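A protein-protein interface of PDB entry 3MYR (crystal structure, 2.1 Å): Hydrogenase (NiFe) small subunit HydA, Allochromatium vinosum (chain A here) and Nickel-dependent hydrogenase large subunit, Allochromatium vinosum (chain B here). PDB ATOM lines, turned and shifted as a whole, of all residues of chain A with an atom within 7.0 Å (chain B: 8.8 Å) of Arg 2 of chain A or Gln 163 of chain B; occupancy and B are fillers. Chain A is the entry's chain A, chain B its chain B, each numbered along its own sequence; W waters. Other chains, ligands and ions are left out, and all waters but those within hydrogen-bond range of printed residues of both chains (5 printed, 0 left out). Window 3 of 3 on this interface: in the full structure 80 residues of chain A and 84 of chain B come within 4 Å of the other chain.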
ATOM      1  N   ALA A   1     -28.220   7.658  -4.451  1.00  0.00           N
ATOM      2  CA  ALA A   1     -27.608   8.633  -3.463  1.00  0.00           C
ATOM      3  C   ALA A   1     -26.889   8.013  -2.198  1.00  0.00           C
ATOM      4  O   ALA A   1     -27.342   7.008  -1.633  1.00  0.00           O
ATOM      5  CB  ALA A   1     -28.615   9.755  -3.043  1.00  0.00           C
ATOM      6  N   ARG A   2     -25.766   8.633  -1.826  1.00  0.00           N
ATOM      7  CA  ARG A   2     -24.849   8.274  -0.711  1.00  0.00           C
ATOM      8  C   ARG A   2     -23.455   8.922  -0.916  1.00  0.00           C
ATOM      9  O   ARG A   2     -22.922   9.410   0.044  1.00  0.00           O
ATOM     10  CB  ARG A   2     -24.695   6.795  -0.430  1.00  0.00           C
ATOM     11  CG  ARG A   2     -23.304   6.432   0.035  1.00  0.00           C
ATOM     12  CD  ARG A   2     -23.264   6.404   1.547  1.00  0.00           C
ATOM     13  NE  ARG A   2     -22.742   5.104   1.969  1.00  0.00           N
ATOM     14  CZ  ARG A   2     -23.309   3.924   1.671  1.00  0.00           C
ATOM     15  NH1 ARG A   2     -24.444   3.861   0.964  1.00  0.00           N
ATOM     16  NH2 ARG A   2     -22.737   2.790   2.074  1.00  0.00           N
ATOM     17  N   ARG A   3     -22.876   8.933  -2.122  1.00  0.00           N
ATOM     18  CA  ARG A   3     -21.852   9.984  -2.467  1.00  0.00           C
ATOM     19  C   ARG A   3     -22.573  11.193  -3.105  1.00  0.00           C
ATOM     20  O   ARG A   3     -23.470  11.020  -3.892  1.00  0.00           O
ATOM     21  CB  ARG A   3     -20.724   9.475  -3.393  1.00  0.00           C
ATOM     22  CG  ARG A   3     -19.700   8.472  -2.738  1.00  0.00           C
ATOM     23  CD  ARG A   3     -18.802   7.869  -3.862  1.00  0.00           C
ATOM     24  NE  ARG A   3     -19.467   6.694  -4.499  1.00  0.00           N
ATOM     25  CZ  ARG A   3     -19.801   6.622  -5.800  1.00  0.00           C
ATOM     26  NH1 ARG A   3     -19.578   7.656  -6.592  1.00  0.00           N
ATOM     27  NH2 ARG A   3     -20.432   5.549  -6.308  1.00  0.00           N
ATOM     28  N   PRO A   4     -22.239  12.419  -2.667  1.00  0.00           N
ATOM     29  CA  PRO A   4     -23.019  13.566  -3.101  1.00  0.00           C
ATOM     30  C   PRO A   4     -22.873  13.771  -4.617  1.00  0.00           C
ATOM     31  O   PRO A   4     -21.774  13.627  -5.176  1.00  0.00           O
ATOM     32  CB  PRO A   4     -22.395  14.746  -2.332  1.00  0.00           C
ATOM     33  CG  PRO A   4     -21.145  14.229  -1.766  1.00  0.00           C
ATOM     34  CD  PRO A   4     -21.310  12.753  -1.575  1.00  0.00           C
ATOM     35  N   SER A   5     -23.969  14.111  -5.251  1.00  0.00           N
ATOM     36  CA  SER A   5     -24.015  14.244  -6.699  1.00  0.00           C
ATOM     37  C   SER A   5     -23.408  15.545  -7.248  1.00  0.00           C
ATOM     38  O   SER A   5     -23.611  16.643  -6.670  1.00  0.00           O
ATOM     39  CB  SER A   5     -25.441  14.128  -7.148  1.00  0.00           C
ATOM     40  OG  SER A   5     -25.542  14.346  -8.552  1.00  0.00           O
ATOM     41  N   ILE A  33     -13.967  10.669  -7.647  1.00  0.00           N
ATOM     42  CA  ILE A  33     -15.005  10.041  -8.422  1.00  0.00           C
ATOM     43  C   ILE A  33     -15.379   8.687  -7.833  1.00  0.00           C
ATOM     44  O   ILE A  33     -16.587   8.302  -7.839  1.00  0.00           O
ATOM     45  CB  ILE A  33     -14.491   9.864  -9.870  1.00  0.00           C
ATOM     46  CG1 ILE A  33     -14.748  11.115 -10.678  1.00  0.00           C
ATOM     47  CG2 ILE A  33     -14.994   8.603 -10.561  1.00  0.00           C
ATOM     48  CD1 ILE A  33     -14.144  10.869 -12.139  1.00  0.00           C
ATOM     49  N   PHE A  36     -15.561   9.972  -3.097  1.00  0.00           N
ATOM     50  CA  PHE A  36     -16.018  11.172  -2.438  1.00  0.00           C
ATOM     51  C   PHE A  36     -17.254  11.786  -3.094  1.00  0.00           C
ATOM     52  O   PHE A  36     -18.103  12.319  -2.405  1.00  0.00           O
ATOM     53  CB  PHE A  36     -14.839  12.171  -2.266  1.00  0.00           C
ATOM     54  CG  PHE A  36     -13.767  11.627  -1.352  1.00  0.00           C
ATOM     55  CD1 PHE A  36     -12.525  11.205  -1.856  1.00  0.00           C
ATOM     56  CD2 PHE A  36     -14.086  11.331   0.023  1.00  0.00           C
ATOM     57  CE1 PHE A  36     -11.558  10.543  -0.987  1.00  0.00           C
ATOM     58  CE2 PHE A  36     -13.141  10.698   0.931  1.00  0.00           C
ATOM     59  CZ  PHE A  36     -11.877  10.282   0.421  1.00  0.00           C
ATOM     60  N   ILE A  37     -17.361  11.732  -4.415  1.00  0.00           N
ATOM     61  CA  ILE A  37     -18.507  12.313  -5.082  1.00  0.00           C
ATOM     62  C   ILE A  37     -19.061  11.320  -6.033  1.00  0.00           C
ATOM     63  O   ILE A  37     -18.455  10.272  -6.294  1.00  0.00           O
ATOM     64  CB  ILE A  37     -18.165  13.628  -5.899  1.00  0.00           C
ATOM     65  CG1 ILE A  37     -17.208  13.334  -7.079  1.00  0.00           C
ATOM     66  CG2 ILE A  37     -17.566  14.651  -5.005  1.00  0.00           C
ATOM     67  CD1 ILE A  37     -16.733  14.612  -7.807  1.00  0.00           C
ATOM     68  N   SER A  38     -20.202  11.679  -6.588  1.00  0.00           N
ATOM     69  CA  SER A  38     -20.734  10.928  -7.681  1.00  0.00           C
ATOM     70  C   SER A  38     -20.793  11.893  -8.841  1.00  0.00           C
ATOM     71  O   SER A  38     -21.664  12.787  -8.870  1.00  0.00           O
ATOM     72  CB  SER A  38     -22.137  10.392  -7.368  1.00  0.00           C
ATOM     73  OG  SER A  38     -22.525   9.479  -8.401  1.00  0.00           O
ATOM     74  N   LEU A  39     -19.784  11.825  -9.704  1.00  0.00           N
ATOM     75  CA  LEU A  39     -19.716  12.766 -10.827  1.00  0.00           C
ATOM     76  C   LEU A  39     -20.658  12.188 -11.890  1.00  0.00           C
ATOM     77  O   LEU A  39     -20.335  11.197 -12.561  1.00  0.00           O
ATOM     78  CB  LEU A  39     -18.270  12.835 -11.371  1.00  0.00           C
ATOM     79  CG  LEU A  39     -18.106  13.630 -12.680  1.00  0.00           C
ATOM     80  CD1 LEU A  39     -18.523  15.144 -12.432  1.00  0.00           C
ATOM     81  CD2 LEU A  39     -16.647  13.572 -13.290  1.00  0.00           C
ATOM     82  N   ASP A  40     -21.851  12.769 -12.025  1.00  0.00           N
ATOM     83  CA  ASP A  40     -22.927  12.105 -12.760  1.00  0.00           C
ATOM     84  C   ASP A  40     -23.060  12.534 -14.214  1.00  0.00           C
ATOM     85  O   ASP A  40     -23.736  11.871 -15.006  1.00  0.00           O
ATOM     86  CB  ASP A  40     -24.228  12.337 -12.034  1.00  0.00           C
ATOM     87  CG  ASP A  40     -24.282  11.595 -10.679  1.00  0.00           C
ATOM     88  OD1 ASP A  40     -24.995  12.065  -9.756  1.00  0.00           O
ATOM     89  OD2 ASP A  40     -23.615  10.529 -10.512  1.00  0.00           O
ATOM     90  N   GLU A  63     -33.104  12.740  -8.758  1.00  0.00           N
ATOM     91  CA  GLU A  63     -32.880  11.952  -7.568  1.00  0.00           C
ATOM     92  C   GLU A  63     -32.183  12.693  -6.448  1.00  0.00           C
ATOM     93  O   GLU A  63     -32.231  12.257  -5.324  1.00  0.00           O
ATOM     94  CB  GLU A  63     -32.085  10.708  -7.954  1.00  0.00           C
ATOM     95  CG  GLU A  63     -32.946   9.895  -8.939  1.00  0.00           C
ATOM     96  CD  GLU A  63     -32.437   8.501  -9.277  1.00  0.00           C
ATOM     97  OE1 GLU A  63     -33.280   7.710  -9.791  1.00  0.00           O
ATOM     98  OE2 GLU A  63     -31.241   8.202  -9.074  1.00  0.00           O
ATOM     99  N   ASN A  64     -31.572  13.839  -6.735  1.00  0.00           N
ATOM    100  CA  ASN A  64     -30.780  14.518  -5.729  1.00  0.00           C
ATOM    101  C   ASN A  64     -31.241  15.939  -5.551  1.00  0.00           C
ATOM    102  O   ASN A  64     -30.450  16.830  -5.184  1.00  0.00           O
ATOM    103  CB  ASN A  64     -29.340  14.513  -6.193  1.00  0.00           C
ATOM    104  CG  ASN A  64     -28.774  13.118  -6.266  1.00  0.00           C
ATOM    105  OD1 ASN A  64     -28.610  12.476  -5.257  1.00  0.00           O
ATOM    106  ND2 ASN A  64     -28.562  12.623  -7.466  1.00  0.00           N
ATOM    107  N   ILE B 155     -13.691  -1.199  -8.641  1.00  0.00           N
ATOM    108  CA  ILE B 155     -14.678  -0.911  -9.684  1.00  0.00           C
ATOM    109  C   ILE B 155     -15.960  -1.663  -9.372  1.00  0.00           C
ATOM    110  O   ILE B 155     -17.087  -1.149  -9.583  1.00  0.00           O
ATOM    111  CB  ILE B 155     -14.164  -1.337 -11.035  1.00  0.00           C
ATOM    112  CG1 ILE B 155     -12.931  -0.522 -11.341  1.00  0.00           C
ATOM    113  CG2 ILE B 155     -15.203  -1.094 -12.136  1.00  0.00           C
ATOM    114  CD1 ILE B 155     -12.093  -1.414 -12.133  1.00  0.00           C
ATOM    115  N   LYS B 156     -15.809  -2.870  -8.875  1.00  0.00           N
ATOM    116  CA  LYS B 156     -16.988  -3.622  -8.462  1.00  0.00           C
ATOM    117  C   LYS B 156     -17.787  -2.905  -7.326  1.00  0.00           C
ATOM    118  O   LYS B 156     -18.982  -2.765  -7.455  1.00  0.00           O
ATOM    119  CB  LYS B 156     -16.585  -5.002  -8.016  1.00  0.00           C
ATOM    120  CG  LYS B 156     -17.732  -5.884  -7.519  1.00  0.00           C
ATOM    121  CD  LYS B 156     -17.280  -7.341  -7.584  1.00  0.00           C
ATOM    122  CE  LYS B 156     -18.452  -8.354  -7.434  1.00  0.00           C
ATOM    123  NZ  LYS B 156     -18.601  -8.621  -5.970  1.00  0.00           N
ATOM    124  N   THR B 157     -17.139  -2.398  -6.274  1.00  0.00           N
ATOM    125  CA  THR B 157     -17.848  -1.629  -5.249  1.00  0.00           C
ATOM    126  C   THR B 157     -18.581  -0.375  -5.874  1.00  0.00           C
ATOM    127  O   THR B 157     -19.785  -0.103  -5.644  1.00  0.00           O
ATOM    128  CB  THR B 157     -16.819  -1.188  -4.217  1.00  0.00           C
ATOM    129  OG1 THR B 157     -16.244  -2.357  -3.632  1.00  0.00           O
ATOM    130  CG2 THR B 157     -17.403  -0.199  -3.107  1.00  0.00           C
ATOM    131  N   PHE B 158     -17.900   0.291  -6.789  1.00  0.00           N
ATOM    132  CA  PHE B 158     -18.482   1.426  -7.459  1.00  0.00           C
ATOM    133  C   PHE B 158     -19.755   1.048  -8.213  1.00  0.00           C
ATOM    134  O   PHE B 158     -20.757   1.757  -8.184  1.00  0.00           O
ATOM    135  CB  PHE B 158     -17.463   1.951  -8.453  1.00  0.00           C
ATOM    136  CG  PHE B 158     -17.871   3.154  -9.136  1.00  0.00           C
ATOM    137  CD1 PHE B 158     -18.374   3.088 -10.437  1.00  0.00           C
ATOM    138  CD2 PHE B 158     -17.671   4.389  -8.545  1.00  0.00           C
ATOM    139  CE1 PHE B 158     -18.714   4.242 -11.141  1.00  0.00           C
ATOM    140  CE2 PHE B 158     -18.053   5.585  -9.252  1.00  0.00           C
ATOM    141  CZ  PHE B 158     -18.532   5.508 -10.535  1.00  0.00           C
ATOM    142  N   VAL B 159     -19.659   0.022  -9.026  1.00  0.00           N
ATOM    143  CA  VAL B 159     -20.762  -0.320  -9.922  1.00  0.00           C
ATOM    144  C   VAL B 159     -21.912  -0.848  -9.065  1.00  0.00           C
ATOM    145  O   VAL B 159     -23.082  -0.571  -9.331  1.00  0.00           O
ATOM    146  CB  VAL B 159     -20.356  -1.409 -10.968  1.00  0.00           C
ATOM    147  CG1 VAL B 159     -21.605  -2.137 -11.536  1.00  0.00           C
ATOM    148  CG2 VAL B 159     -19.498  -0.829 -12.096  1.00  0.00           C
ATOM    149  N   GLU B 160     -21.586  -1.541  -7.987  1.00  0.00           N
ATOM    150  CA  GLU B 160     -22.641  -2.087  -7.154  1.00  0.00           C
ATOM    151  C   GLU B 160     -23.304  -1.040  -6.255  1.00  0.00           C
ATOM    152  O   GLU B 160     -24.368  -1.311  -5.724  1.00  0.00           O
ATOM    153  CB  GLU B 160     -22.159  -3.313  -6.355  1.00  0.00           C
ATOM    154  CG  GLU B 160     -22.197  -4.568  -7.262  1.00  0.00           C
ATOM    155  CD  GLU B 160     -21.462  -5.791  -6.701  1.00  0.00           C
ATOM    156  OE1 GLU B 160     -21.248  -6.735  -7.532  1.00  0.00           O
ATOM    157  OE2 GLU B 160     -21.101  -5.809  -5.475  1.00  0.00           O
ATOM    158  N   SER B 161     -22.677   0.128  -6.063  1.00  0.00           N
ATOM    159  CA  SER B 161     -23.248   1.172  -5.202  1.00  0.00           C
ATOM    160  C   SER B 161     -24.566   1.694  -5.858  1.00  0.00           C
ATOM    161  O   SER B 161     -25.267   2.451  -5.235  1.00  0.00           O
ATOM    162  CB  SER B 161     -22.292   2.346  -5.107  1.00  0.00           C
ATOM    163  OG  SER B 161     -22.244   3.012  -6.395  1.00  0.00           O
ATOM    164  N   GLY B 162     -24.815   1.370  -7.130  1.00  0.00           N
ATOM    165  CA  GLY B 162     -25.874   1.993  -7.905  1.00  0.00           C
ATOM    166  C   GLY B 162     -25.649   3.468  -8.301  1.00  0.00           C
ATOM    167  O   GLY B 162     -26.515   4.047  -8.942  1.00  0.00           O
ATOM    168  N   GLN B 163     -24.513   4.090  -7.985  1.00  0.00           N
ATOM    169  CA  GLN B 163     -24.243   5.415  -8.571  1.00  0.00           C
ATOM    170  C   GLN B 163     -23.126   5.237  -9.583  1.00  0.00           C
ATOM    171  O   GLN B 163     -21.907   5.314  -9.228  1.00  0.00           O
ATOM    172  CB  GLN B 163     -23.840   6.439  -7.480  1.00  0.00           C
ATOM    173  CG  GLN B 163     -24.972   6.794  -6.486  1.00  0.00           C
ATOM    174  CD  GLN B 163     -24.498   7.725  -5.405  1.00  0.00           C
ATOM    175  OE1 GLN B 163     -23.823   7.316  -4.464  1.00  0.00           O
ATOM    176  NE2 GLN B 163     -24.735   8.996  -5.598  1.00  0.00           N
ATOM    177  N   LEU B 164     -23.514   5.040 -10.842  1.00  0.00           N
ATOM    178  CA  LEU B 164     -22.556   4.648 -11.851  1.00  0.00           C
ATOM    179  C   LEU B 164     -21.796   5.821 -12.454  1.00  0.00           C
ATOM    180  O   LEU B 164     -20.839   5.583 -13.193  1.00  0.00           O
ATOM    181  CB  LEU B 164     -23.191   3.822 -12.966  1.00  0.00           C
ATOM    182  CG  LEU B 164     -23.067   2.302 -12.639  1.00  0.00           C
ATOM    183  CD1 LEU B 164     -24.017   2.023 -11.488  1.00  0.00           C
ATOM    184  CD2 LEU B 164     -23.474   1.412 -13.793  1.00  0.00           C
ATOM    185  N   GLY B 165     -22.198   7.054 -12.124  1.00  0.00           N
ATOM    186  CA  GLY B 165     -21.403   8.248 -12.490  1.00  0.00           C
ATOM    187  C   GLY B 165     -21.254   8.263 -14.020  1.00  0.00           C
ATOM    188  O   GLY B 165     -22.235   8.089 -14.748  1.00  0.00           O
ATOM    189  N   ILE B 166     -20.023   8.379 -14.499  1.00  0.00           N
ATOM    190  CA  ILE B 166     -19.758   8.540 -15.920  1.00  0.00           C
ATOM    191  C   ILE B 166     -19.950   7.227 -16.694  1.00  0.00           C
ATOM    192  O   ILE B 166     -19.868   7.223 -17.920  1.00  0.00           O
ATOM    193  CB  ILE B 166     -18.287   9.051 -16.177  1.00  0.00           C
ATOM    194  CG1 ILE B 166     -17.281   8.020 -15.671  1.00  0.00           C
ATOM    195  CG2 ILE B 166     -18.086  10.458 -15.518  1.00  0.00           C
ATOM    196  CD1 ILE B 166     -15.768   8.331 -16.049  1.00  0.00           C
ATOM    197  N   PHE B 167     -20.156   6.135 -15.974  1.00  0.00           N
ATOM    198  CA  PHE B 167     -20.471   4.849 -16.588  1.00  0.00           C
ATOM    199  C   PHE B 167     -21.970   4.589 -16.753  1.00  0.00           C
ATOM    200  O   PHE B 167     -22.342   3.579 -17.359  1.00  0.00           O
ATOM    201  CB  PHE B 167     -19.899   3.662 -15.782  1.00  0.00           C
ATOM    202  CG  PHE B 167     -18.397   3.637 -15.670  1.00  0.00           C
ATOM    203  CD1 PHE B 167     -17.599   4.291 -16.590  1.00  0.00           C
ATOM    204  CD2 PHE B 167     -17.790   2.790 -14.738  1.00  0.00           C
ATOM    205  CE1 PHE B 167     -16.202   4.270 -16.485  1.00  0.00           C
ATOM    206  CE2 PHE B 167     -16.397   2.716 -14.666  1.00  0.00           C
ATOM    207  CZ  PHE B 167     -15.610   3.491 -15.539  1.00  0.00           C
ATOM    208  N   ALA B 168     -22.819   5.444 -16.186  1.00  0.00           N
ATOM    209  CA  ALA B 168     -24.280   5.234 -16.237  1.00  0.00           C
ATOM    210  C   ALA B 168     -24.843   5.258 -17.668  1.00  0.00           C
ATOM    211  O   ALA B 168     -24.397   6.084 -18.489  1.00  0.00           O
ATOM    212  CB  ALA B 168     -25.009   6.306 -15.344  1.00  0.00           C
HETATM  213  O   HOH W   1     -24.495   8.013 -10.826  1.00  0.00           O
HETATM  214  O   HOH W   2     -20.729   7.802  -9.156  1.00  0.00           O
HETATM  215  O   HOH W   3     -18.233   9.359 -12.297  1.00  0.00           O
HETATM  216  O   HOH W   4     -25.934  10.329  -7.983  1.00  0.00           O
HETATM  217  O   HOH W   5     -24.577   9.401 -14.301  1.00  0.00           O
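NH2 of Arg 3 of chain A is in hydrogen-bond range of OG of Ser 161 of chain B. The backbone carbonyl oxygen (O) of Arg 3 of chain A is in hydrogen-bond range of the side-chain amide nitrogen (NE2) of Gln 163 of chain B. N of Ile 166 of chain B is in hydrogen-bond range of O of Leu 39 of chain A (3.4 Å).
NH1 of Arg 3 of chain A is in hydrogen-bond range of O of Ile 33 of chain A (3.3 Å). The backbone carbonyl oxygen of Ile 37 of chain A sits at hydrogen-bond distance from the guanidinium group of Arg 3 of chain A (2.9 Å). O of Pro 4 of chain A lies within hydrogen-bond range of N of Ser 38 of chain A. OG of Ser 5 of chain A sits at hydrogen-bond distance from OD1 of Asp 40 of chain A (2.6 Å). The side-chain hydroxyl of Ser 161 of chain B lies within hydrogen-bond range of the backbone carbonyl oxygen of Phe 158 of chain B (2.6 Å). OG of Ser 161 of chain B is in hydrogen-bond range of N of Gln 163 of chain B.
Ala 1 of chain A touches Gln 163 of chain B. Arg 2 of chain A touches Gln 163 of chain B. NH1 of Arg 3 of chain A touches CE2 of Phe 158 of chain B, 3.7 Å away. Phe 158 of chain B touches Ile 33 of chain A. Ser 38 of chain A touches Gln 163 of chain B (OG to CB, 3.4 Å). O of Leu 39 of chain A touches CA of Gly 165 of chain B (3.1 Å). Gly 165 of chain B touches Asp 40 of chain A (CA to OD2, 3.7 Å).
Of chain B, only Gln 163 comes within 4 Å of Ala 1 of chain A. Arg 2 of chain A touches one residue of chain B. Of the printed residues of chain B, Asp 40 of chain A touches Gly 165 (3.7 Å). Ile 155 of chain B touches none of the printed residues of chain A. Gly 162 of chain B touches none of the printed residues of chain A. Of chain A, only Ala 1 (3.6 Å), Arg 2 (3.5 Å), Arg 3 (2.9 Å) and Ser 38 (3.4 Å) come within 4 Å of Gln 163 of chain B. Printed residues of chain A within 4 Å of Ile 166 of chain B: Leu 39 (3.4 Å). The nearest printed residue of chain A that does not touch Ile 166 of chain B is Ile 33 of chain A (4.9 Å).
Of the 13 printed residues of chain A, 7 touch a printed residue of chain B. Printed residues of chain A that touch a printed residue of chain B: Ala 1, Arg 2, Arg 3, Ile 33, Ser 38, Leu 39 and Asp 40. Of the 14 printed residues of chain B, 5 touch a printed residue of chain A. Hydrophobic or aromatic side chains of chain B that line the printed part of chain A: Phe 158 and Ile 166.
Water W2 lies within hydrogen-bond range of OG of Ser 38 of chain A (2.6 Å), O of Gln 163 of chain B (2.8 Å), NH1 of Arg 3 of chain A (2.8 Å) and N of Gly 165 of chain B (3.4 Å). Water W4 bridges OD1 of Asp 40 of chain A (2.7 Å) and NE2 of Gln 163 of chain B (3.0 Å). Water W1 lies within hydrogen-bond range of OD2 of Asp 40 of chain A (2.7 Å), N of Gly 165 of chain B (2.8 Å), N of Leu 164 of chain B (3.1 Å) and OG of Ser 38 of chain A (3.5 Å). Water W5 lies within hydrogen-bond range of the backbone carbonyl oxygen of Asp 40 of chain A (2.7 Å) and the backbone carbonyl oxygen of Gly 165 of chain B (2.7 Å). Water W3 lies within hydrogen-bond range of O of Leu 39 of chain A and N of Ile 166 of chain B.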
